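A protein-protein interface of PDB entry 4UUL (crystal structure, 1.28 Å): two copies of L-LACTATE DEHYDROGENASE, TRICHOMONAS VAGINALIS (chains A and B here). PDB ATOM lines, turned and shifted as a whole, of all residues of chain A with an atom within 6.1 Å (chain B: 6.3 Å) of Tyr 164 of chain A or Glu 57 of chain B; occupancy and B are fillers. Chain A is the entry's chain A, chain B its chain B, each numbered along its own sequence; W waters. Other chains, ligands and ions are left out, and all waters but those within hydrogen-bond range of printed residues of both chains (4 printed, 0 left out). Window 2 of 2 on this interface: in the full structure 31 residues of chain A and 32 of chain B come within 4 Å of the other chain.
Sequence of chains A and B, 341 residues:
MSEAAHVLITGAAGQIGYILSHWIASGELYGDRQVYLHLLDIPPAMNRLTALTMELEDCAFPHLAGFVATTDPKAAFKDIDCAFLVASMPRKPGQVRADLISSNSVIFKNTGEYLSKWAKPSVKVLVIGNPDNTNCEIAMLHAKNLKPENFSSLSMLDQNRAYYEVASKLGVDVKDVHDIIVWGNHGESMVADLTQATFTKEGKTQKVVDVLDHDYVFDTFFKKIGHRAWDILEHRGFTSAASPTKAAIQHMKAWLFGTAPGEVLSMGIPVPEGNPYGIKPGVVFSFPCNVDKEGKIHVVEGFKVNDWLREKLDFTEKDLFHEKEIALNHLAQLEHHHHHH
Water W2 lies within hydrogen-bond range of the side-chain carboxylate of Glu 57 of chain B (2.5 Å), the guanidinium group of Arg 228 of chain A (3.0 Å) and the side-chain hydroxyl of Tyr 164 of chain A (3.3 Å).
Water W4 lies within hydrogen-bond range of the side-chain carboxylate of Asp 58 of chain B (2.7 Å) and the guanidinium group of Arg 161 of chain A (2.9 Å).
Water W3 bridges OD1 of Asp 58 of chain B and O of Arg 161 of chain A.
Water W1 bridges the backbone carbonyl oxygen of Asp 58 of chain B and the side-chain amide nitrogen of Asn 160 of chain A.
NE of Arg 161 of chain A lies within salt-bridge range of OD2 of Asp 58 of chain B, 3.2 Å away.
OH of Tyr 164 of chain A lies within hydrogen-bond range of OE2 of Glu 57 of chain B (3.1 Å).
The guanidinium group of Arg 228 of chain A is in hydrogen-bond range of the backbone carbonyl oxygen of Met 54 of chain B.
OE1 of Glu 57 of chain B lies within salt-bridge range of NH2 of Arg 228 of chain A (2.9 Å).
NH2 of Arg 228 of chain A lies within salt-bridge range of OD1 of Asp 58 of chain B, 2.9 Å away.
CB of Asn 160 of chain A touches O of Asp 58 of chain B, at 3.2 Å.
O of Cys 59 of chain B touches ND2 of Asn 160 of chain A, at 3.7 Å.
Ala 60 of chain B touches Asn 160 of chain A.
No position is printed for both chains.
Of the 8 pairs that touch across the chains among the printed residues, none has its exchanged pair printed and touching as well.
Hydrophobic or aromatic side chains of chain A within 4 Å of the printed part of chain B: Tyr 164.
Among the printed residues, 8 pairs touch across the chains.
The backbone carbonyl oxygen (O) of Tyr 164 of chain A sits at hydrogen-bond distance from the side-chain hydroxyl (OG) of Ser 168 of chain A, 3.4 Å away.
O of Glu 55 of chain B is in hydrogen-bond range of SG of Cys 59 of chain B (3.4 Å).
Printed residues of chain A within 4 Å of Glu 57 of chain B: Tyr 164 (3.1 Å) and Arg 228 (2.9 Å).
Of the printed residues of chain B, Arg 161 of chain A touches Asp 58.
Printed residues of chain A within 4 Å of Ala 60 of chain B: Asn 160.
Of the printed residues of chain B, Asn 160 of chain A touches Asp 58, Cys 59 and Ala 60.
Of the printed residues of chain A, Met 54 of chain B touches Arg 228.
Of the printed residues of chain A, Cys 59 of chain B touches Asn 160 (3.7 Å).
The nearest printed residue of chain A that does not touch Glu 57 of chain B is Asn 160 of chain A (4.5 Å).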
ATOM      1  N   GLN A 159     -19.861  -6.923  25.439  1.00  0.00           N
ATOM      2  CA  GLN A 159     -20.632  -5.926  24.691  1.00  0.00           C
ATOM      3  C   GLN A 159     -19.768  -5.306  23.599  1.00  0.00           C
ATOM      4  O   GLN A 159     -20.193  -5.181  22.451  1.00  0.00           O
ATOM      5  CB  GLN A 159     -21.212  -4.851  25.591  1.00  0.00           C
ATOM      6  CG  GLN A 159     -21.911  -3.781  24.826  1.00  0.00           C
ATOM      7  CD  GLN A 159     -22.667  -2.796  25.677  1.00  0.00           C
ATOM      8  OE1 GLN A 159     -23.458  -3.175  26.526  1.00  0.00           O
ATOM      9  NE2 GLN A 159     -22.501  -1.519  25.420  1.00  0.00           N
ATOM     10  N   ASN A 160     -18.556  -4.884  23.942  1.00  0.00           N
ATOM     11  CA  ASN A 160     -17.664  -4.249  22.973  1.00  0.00           C
ATOM     12  C   ASN A 160     -17.336  -5.220  21.834  1.00  0.00           C
ATOM     13  O   ASN A 160     -17.348  -4.819  20.661  1.00  0.00           O
ATOM     14  CB  ASN A 160     -16.399  -3.761  23.680  1.00  0.00           C
ATOM     15  CG  ASN A 160     -16.662  -2.510  24.499  1.00  0.00           C
ATOM     16  OD1 ASN A 160     -17.617  -1.767  24.224  1.00  0.00           O
ATOM     17  ND2 ASN A 160     -15.822  -2.238  25.484  1.00  0.00           N
ATOM     18  N   ARG A 161     -17.055  -6.493  22.146  1.00  0.00           N
ATOM     19  CA  ARG A 161     -16.815  -7.494  21.108  1.00  0.00           C
ATOM     20  C   ARG A 161     -18.028  -7.592  20.175  1.00  0.00           C
ATOM     21  O   ARG A 161     -17.870  -7.668  18.952  1.00  0.00           O
ATOM     22  CB  ARG A 161     -16.572  -8.842  21.749  1.00  0.00           C
ATOM     23  CG  ARG A 161     -15.214  -9.010  22.374  1.00  0.00           C
ATOM     24  CD  ARG A 161     -15.078 -10.355  23.048  1.00  0.00           C
ATOM     25  NE  ARG A 161     -13.722 -10.607  23.484  1.00  0.00           N
ATOM     26  CZ  ARG A 161     -13.385 -11.455  24.425  1.00  0.00           C
ATOM     27  NH1 ARG A 161     -14.350 -12.133  25.071  1.00  0.00           N
ATOM     28  NH2 ARG A 161     -12.111 -11.636  24.728  1.00  0.00           N
ATOM     29  N   ALA A 162     -19.223  -7.575  20.741  1.00  0.00           N
ATOM     30  CA  ALA A 162     -20.424  -7.720  19.939  1.00  0.00           C
ATOM     31  C   ALA A 162     -20.648  -6.512  19.024  1.00  0.00           C
ATOM     32  O   ALA A 162     -21.013  -6.669  17.850  1.00  0.00           O
ATOM     33  CB  ALA A 162     -21.644  -7.936  20.865  1.00  0.00           C
ATOM     34  N   TYR A 163     -20.407  -5.304  19.534  1.00  0.00           N
ATOM     35  CA  TYR A 163     -20.517  -4.123  18.700  1.00  0.00           C
ATOM     36  C   TYR A 163     -19.574  -4.161  17.504  1.00  0.00           C
ATOM     37  O   TYR A 163     -19.968  -3.846  16.395  1.00  0.00           O
ATOM     38  CB  TYR A 163     -20.313  -2.852  19.499  1.00  0.00           C
ATOM     39  CG  TYR A 163     -21.571  -2.242  20.079  1.00  0.00           C
ATOM     40  CD1 TYR A 163     -22.356  -1.401  19.326  1.00  0.00           C
ATOM     41  CD2 TYR A 163     -21.980  -2.506  21.378  1.00  0.00           C
ATOM     42  CE1 TYR A 163     -23.502  -0.834  19.852  1.00  0.00           C
ATOM     43  CE2 TYR A 163     -23.143  -1.918  21.922  1.00  0.00           C
ATOM     44  CZ  TYR A 163     -23.889  -1.107  21.155  1.00  0.00           C
ATOM     45  OH  TYR A 163     -25.012  -0.501  21.645  1.00  0.00           O
ATOM     46  N   TYR A 164     -18.312  -4.522  17.762  1.00  0.00           N
ATOM     47  CA  TYR A 164     -17.340  -4.628  16.676  1.00  0.00           C
ATOM     48  C   TYR A 164     -17.864  -5.571  15.611  1.00  0.00           C
ATOM     49  O   TYR A 164     -17.947  -5.224  14.431  1.00  0.00           O
ATOM     50  CB  TYR A 164     -15.987  -5.167  17.152  1.00  0.00           C
ATOM     51  CG  TYR A 164     -15.262  -5.818  15.973  1.00  0.00           C
ATOM     52  CD1 TYR A 164     -14.750  -5.040  14.951  1.00  0.00           C
ATOM     53  CD2 TYR A 164     -15.148  -7.203  15.869  1.00  0.00           C
ATOM     54  CE1 TYR A 164     -14.170  -5.627  13.834  1.00  0.00           C
ATOM     55  CE2 TYR A 164     -14.554  -7.804  14.794  1.00  0.00           C
ATOM     56  CZ  TYR A 164     -14.053  -7.005  13.769  1.00  0.00           C
ATOM     57  OH  TYR A 164     -13.478  -7.616  12.686  1.00  0.00           O
ATOM     58  N   GLU A 165     -18.222  -6.773  16.050  1.00  0.00           N
ATOM     59  CA  GLU A 165     -18.606  -7.855  15.144  1.00  0.00           C
ATOM     60  C   GLU A 165     -19.792  -7.431  14.282  1.00  0.00           C
ATOM     61  O   GLU A 165     -19.793  -7.629  13.086  1.00  0.00           O
ATOM     62  CB  GLU A 165     -18.945  -9.089  15.975  1.00  0.00           C
ATOM     63  CG  GLU A 165     -19.584 -10.226  15.208  1.00  0.00           C
ATOM     64  CD  GLU A 165     -18.750 -10.745  14.056  1.00  0.00           C
ATOM     65  OE1 GLU A 165     -17.499 -10.692  14.096  1.00  0.00           O
ATOM     66  OE2 GLU A 165     -19.352 -11.240  13.087  1.00  0.00           O
ATOM     67  N   VAL A 166     -20.818  -6.878  14.895  1.00  0.00           N
ATOM     68  CA  VAL A 166     -22.004  -6.498  14.167  1.00  0.00           C
ATOM     69  C   VAL A 166     -21.733  -5.317  13.219  1.00  0.00           C
ATOM     70  O   VAL A 166     -22.178  -5.339  12.069  1.00  0.00           O
ATOM     71  CB  VAL A 166     -23.163  -6.171  15.122  1.00  0.00           C
ATOM     72  CG1 VAL A 166     -24.401  -5.579  14.364  1.00  0.00           C
ATOM     73  CG2 VAL A 166     -23.596  -7.424  15.852  1.00  0.00           C
ATOM     74  N   ALA A 167     -21.014  -4.307  13.665  1.00  0.00           N
ATOM     75  CA  ALA A 167     -20.691  -3.167  12.818  1.00  0.00           C
ATOM     76  C   ALA A 167     -19.885  -3.652  11.622  1.00  0.00           C
ATOM     77  O   ALA A 167     -20.134  -3.232  10.487  1.00  0.00           O
ATOM     78  CB  ALA A 167     -19.918  -2.151  13.597  1.00  0.00           C
ATOM     79  N   SER A 168     -18.936  -4.558  11.852  1.00  0.00           N
ATOM     80  CA  SER A 168     -18.120  -5.065  10.741  1.00  0.00           C
ATOM     81  C   SER A 168     -18.980  -5.893   9.758  1.00  0.00           C
ATOM     82  O   SER A 168     -18.838  -5.787   8.550  1.00  0.00           O
ATOM     83  CB  SER A 168     -16.923  -5.842  11.247  1.00  0.00           C
ATOM     84  OG  SER A 168     -17.256  -7.112  11.747  1.00  0.00           O
ATOM     85  N   LYS A 169     -19.931  -6.665  10.269  1.00  0.00           N
ATOM     86  CA  LYS A 169     -20.758  -7.492   9.402  1.00  0.00           C
ATOM     87  C   LYS A 169     -21.648  -6.599   8.550  1.00  0.00           C
ATOM     88  O   LYS A 169     -21.901  -6.891   7.377  1.00  0.00           O
ATOM     89  CB  LYS A 169     -21.592  -8.419  10.278  1.00  0.00           C
ATOM     90  CG  LYS A 169     -22.594  -9.267   9.533  1.00  0.00           C
ATOM     91  CD  LYS A 169     -21.900 -10.316   8.661  1.00  0.00           C
ATOM     92  CE  LYS A 169     -22.932 -11.272   8.076  1.00  0.00           C
ATOM     93  NZ  LYS A 169     -22.274 -12.433   7.471  1.00  0.00           N
ATOM     94  N   VAL A 174     -18.890   1.568  14.341  1.00  0.00           N
ATOM     95  CA  VAL A 174     -19.473   1.138  15.603  1.00  0.00           C
ATOM     96  C   VAL A 174     -20.471   2.170  16.124  1.00  0.00           C
ATOM     97  O   VAL A 174     -21.489   1.832  16.721  1.00  0.00           O
ATOM     98  CB  VAL A 174     -18.370   0.827  16.623  1.00  0.00           C
ATOM     99  CG1 VAL A 174     -18.903   0.770  18.024  1.00  0.00           C
ATOM    100  CG2 VAL A 174     -17.696  -0.493  16.323  1.00  0.00           C
ATOM    101  N   ARG A 228     -14.107 -16.070  20.682  1.00  0.00           N
ATOM    102  CA  ARG A 228     -13.220 -14.937  20.471  1.00  0.00           C
ATOM    103  C   ARG A 228     -11.981 -14.952  21.387  1.00  0.00           C
ATOM    104  O   ARG A 228     -10.846 -14.735  20.946  1.00  0.00           O
ATOM    105  CB  ARG A 228     -14.005 -13.646  20.715  1.00  0.00           C
ATOM    106  CG  ARG A 228     -13.222 -12.405  20.414  1.00  0.00           C
ATOM    107  CD  ARG A 228     -12.696 -12.407  18.970  1.00  0.00           C
ATOM    108  NE  ARG A 228     -12.290 -11.038  18.615  1.00  0.00           N
ATOM    109  CZ  ARG A 228     -12.049 -10.586  17.385  1.00  0.00           C
ATOM    110  NH1 ARG A 228     -12.080 -11.381  16.309  1.00  0.00           N
ATOM    111  NH2 ARG A 228     -11.747  -9.313  17.226  1.00  0.00           N
ATOM    112  N   HIS B  22      -3.130   0.529  21.774  1.00  0.00           N
ATOM    113  CA  HIS B  22      -4.377   0.706  22.504  1.00  0.00           C
ATOM    114  C   HIS B  22      -4.521   2.111  23.105  1.00  0.00           C
ATOM    115  O   HIS B  22      -5.592   2.710  23.076  1.00  0.00           O
ATOM    116  CB  HIS B  22      -4.505  -0.351  23.602  1.00  0.00           C
ATOM    117  CG  HIS B  22      -4.934  -1.705  23.126  1.00  0.00           C
ATOM    118  ND1 HIS B  22      -4.062  -2.644  22.637  1.00  0.00           N
ATOM    119  CD2 HIS B  22      -6.165  -2.278  23.071  1.00  0.00           C
ATOM    120  CE1 HIS B  22      -4.747  -3.721  22.273  1.00  0.00           C
ATOM    121  NE2 HIS B  22      -6.016  -3.515  22.521  1.00  0.00           N
ATOM    122  N   LEU B  52      -3.124  -8.712  18.394  1.00  0.00           N
ATOM    123  CA  LEU B  52      -3.233  -7.295  18.786  1.00  0.00           C
ATOM    124  C   LEU B  52      -4.449  -6.665  18.121  1.00  0.00           C
ATOM    125  O   LEU B  52      -5.238  -6.002  18.758  1.00  0.00           O
ATOM    126  CB  LEU B  52      -1.943  -6.497  18.482  1.00  0.00           C
ATOM    127  CG  LEU B  52      -2.161  -4.971  18.349  1.00  0.00           C
ATOM    128  CD1 LEU B  52      -2.582  -4.434  19.652  1.00  0.00           C
ATOM    129  CD2 LEU B  52      -0.852  -4.308  17.920  1.00  0.00           C
ATOM    130  N   THR B  53      -4.581  -6.852  16.811  1.00  0.00           N
ATOM    131  CA  THR B  53      -5.681  -6.205  16.122  1.00  0.00           C
ATOM    132  C   THR B  53      -7.023  -6.727  16.592  1.00  0.00           C
ATOM    133  O   THR B  53      -8.004  -5.974  16.633  1.00  0.00           O
ATOM    134  CB  THR B  53      -5.574  -6.237  14.603  1.00  0.00           C
ATOM    135  OG1 THR B  53      -5.676  -7.568  14.133  1.00  0.00           O
ATOM    136  CG2 THR B  53      -4.259  -5.613  14.150  1.00  0.00           C
ATOM    137  N   MET B  54      -7.084  -8.000  16.966  1.00  0.00           N
ATOM    138  CA  MET B  54      -8.346  -8.536  17.469  1.00  0.00           C
ATOM    139  C   MET B  54      -8.708  -7.832  18.792  1.00  0.00           C
ATOM    140  O   MET B  54      -9.897  -7.543  19.053  1.00  0.00           O
ATOM    141  CB  MET B  54      -8.173  -9.998  17.700  1.00  0.00           C
ATOM    142  CG  MET B  54      -8.174 -10.825  16.445  1.00  0.00           C
ATOM    143  SD  MET B  54      -7.675 -12.568  16.723  1.00  0.00           S
ATOM    144  CE  MET B  54      -9.214 -13.302  17.204  1.00  0.00           C
ATOM    145  N   GLU B  55      -7.734  -7.595  19.665  1.00  0.00           N
ATOM    146  CA  GLU B  55      -8.018  -6.851  20.885  1.00  0.00           C
ATOM    147  C   GLU B  55      -8.378  -5.423  20.625  1.00  0.00           C
ATOM    148  O   GLU B  55      -9.305  -4.898  21.293  1.00  0.00           O
ATOM    149  CB  GLU B  55      -6.920  -6.976  21.927  1.00  0.00           C
ATOM    150  CG  GLU B  55      -6.876  -8.354  22.542  1.00  0.00           C
ATOM    151  CD  GLU B  55      -6.133  -8.341  23.845  1.00  0.00           C
ATOM    152  OE1 GLU B  55      -6.682  -7.810  24.849  1.00  0.00           O
ATOM    153  OE2 GLU B  55      -4.965  -8.806  23.880  1.00  0.00           O
ATOM    154  N   LEU B  56      -7.729  -4.787  19.654  1.00  0.00           N
ATOM    155  CA  LEU B  56      -8.147  -3.430  19.304  1.00  0.00           C
ATOM    156  C   LEU B  56      -9.604  -3.414  18.879  1.00  0.00           C
ATOM    157  O   LEU B  56     -10.387  -2.581  19.337  1.00  0.00           O
ATOM    158  CB  LEU B  56      -7.280  -2.857  18.199  1.00  0.00           C
ATOM    159  CG  LEU B  56      -5.823  -2.582  18.490  1.00  0.00           C
ATOM    160  CD1 LEU B  56      -5.101  -2.175  17.196  1.00  0.00           C
ATOM    161  CD2 LEU B  56      -5.686  -1.446  19.485  1.00  0.00           C
ATOM    162  N   GLU B  57      -9.971  -4.354  17.999  1.00  0.00           N
ATOM    163  CA  GLU B  57     -11.368  -4.491  17.582  1.00  0.00           C
ATOM    164  C   GLU B  57     -12.314  -4.630  18.759  1.00  0.00           C
ATOM    165  O   GLU B  57     -13.358  -3.970  18.817  1.00  0.00           O
ATOM    166  CB  GLU B  57     -11.506  -5.684  16.623  1.00  0.00           C
ATOM    167  CG  GLU B  57     -10.868  -5.420  15.307  1.00  0.00           C
ATOM    168  CD  GLU B  57     -10.816  -6.636  14.378  1.00  0.00           C
ATOM    169  OE1 GLU B  57     -10.991  -7.768  14.850  1.00  0.00           O
ATOM    170  OE2 GLU B  57     -10.665  -6.434  13.155  1.00  0.00           O
ATOM    171  N   ASP B  58     -11.923  -5.473  19.696  1.00  0.00           N
ATOM    172  CA  ASP B  58     -12.753  -5.832  20.831  1.00  0.00           C
ATOM    173  C   ASP B  58     -12.837  -4.734  21.910  1.00  0.00           C
ATOM    174  O   ASP B  58     -13.549  -4.896  22.924  1.00  0.00           O
ATOM    175  CB  ASP B  58     -12.181  -7.077  21.509  1.00  0.00           C
ATOM    176  CG  ASP B  58     -12.400  -8.336  20.701  1.00  0.00           C
ATOM    177  OD1 ASP B  58     -13.076  -8.261  19.635  1.00  0.00           O
ATOM    178  OD2 ASP B  58     -11.961  -9.422  21.155  1.00  0.00           O
ATOM    179  N   CYS B  59     -12.193  -3.610  21.665  1.00  0.00           N
ATOM    180  CA  CYS B  59     -12.398  -2.433  22.513  1.00  0.00           C
ATOM    181  C   CYS B  59     -13.523  -1.535  21.976  1.00  0.00           C
ATOM    182  O   CYS B  59     -13.932  -0.631  22.688  1.00  0.00           O
ATOM    183  CB  CYS B  59     -11.102  -1.625  22.616  1.00  0.00           C
ATOM    184  SG  CYS B  59      -9.826  -2.457  23.582  1.00  0.00           S
ATOM    185  N   ALA B  60     -13.917  -1.693  20.715  1.00  0.00           N
ATOM    186  CA  ALA B  60     -14.951  -0.837  20.127  1.00  0.00           C
ATOM    187  C   ALA B  60     -14.617   0.623  20.341  1.00  0.00           C
ATOM    188  O   ALA B  60     -15.435   1.434  20.742  1.00  0.00           O
ATOM    189  CB  ALA B  60     -16.356  -1.219  20.659  1.00  0.00           C
ATOM    190  N   PHE B  61     -13.376   0.999  20.026  1.00  0.00           N
ATOM    191  CA  PHE B  61     -12.893   2.360  20.255  1.00  0.00           C
ATOM    192  C   PHE B  61     -13.569   3.346  19.303  1.00  0.00           C
ATOM    193  O   PHE B  61     -13.388   3.224  18.099  1.00  0.00           O
ATOM    194  CB  PHE B  61     -11.392   2.419  19.970  1.00  0.00           C
ATOM    195  CG  PHE B  61     -10.509   1.861  21.039  1.00  0.00           C
ATOM    196  CD1 PHE B  61     -10.546   2.350  22.331  1.00  0.00           C
ATOM    197  CD2 PHE B  61      -9.590   0.886  20.717  1.00  0.00           C
ATOM    198  CE1 PHE B  61      -9.633   1.906  23.321  1.00  0.00           C
ATOM    199  CE2 PHE B  61      -8.670   0.443  21.683  1.00  0.00           C
ATOM    200  CZ  PHE B  61      -8.698   0.966  22.981  1.00  0.00           C
ATOM    201  N   LEU B  64     -11.018   4.951  16.774  1.00  0.00           N
ATOM    202  CA  LEU B  64     -10.284   4.121  15.841  1.00  0.00           C
ATOM    203  C   LEU B  64     -11.008   4.018  14.526  1.00  0.00           C
ATOM    204  O   LEU B  64     -11.999   3.322  14.403  1.00  0.00           O
ATOM    205  CB  LEU B  64      -9.990   2.747  16.433  1.00  0.00           C
ATOM    206  CG  LEU B  64      -9.069   1.826  15.615  1.00  0.00           C
ATOM    207  CD1 LEU B  64      -7.691   2.421  15.395  1.00  0.00           C
ATOM    208  CD2 LEU B  64      -8.902   0.495  16.307  1.00  0.00           C
ATOM    209  N   PHE B  67      -7.275   0.301  10.774  1.00  0.00           N
ATOM    210  CA  PHE B  67      -5.889  -0.071  10.925  1.00  0.00           C
ATOM    211  C   PHE B  67      -5.503  -0.987   9.762  1.00  0.00           C
ATOM    212  O   PHE B  67      -6.356  -1.569   9.076  1.00  0.00           O
ATOM    213  CB  PHE B  67      -5.664  -0.816  12.243  1.00  0.00           C
ATOM    214  CG  PHE B  67      -6.473  -2.062  12.365  1.00  0.00           C
ATOM    215  CD1 PHE B  67      -6.029  -3.252  11.841  1.00  0.00           C
ATOM    216  CD2 PHE B  67      -7.694  -2.036  12.997  1.00  0.00           C
ATOM    217  CE1 PHE B  67      -6.814  -4.408  11.922  1.00  0.00           C
ATOM    218  CE2 PHE B  67      -8.469  -3.171  13.086  1.00  0.00           C
ATOM    219  CZ  PHE B  67      -8.017  -4.356  12.557  1.00  0.00           C
HETATM  220  O   HOH W   1     -13.396  -3.938  25.634  1.00  0.00           O
HETATM  221  O   HOH W   2     -11.449 -10.014  13.751  1.00  0.00           O
HETATM  222  O   HOH W   3     -15.402  -9.228  18.279  1.00  0.00           O
HETATM  223  O   HOH W   4     -10.550  -9.549  23.473  1.00  0.00           O
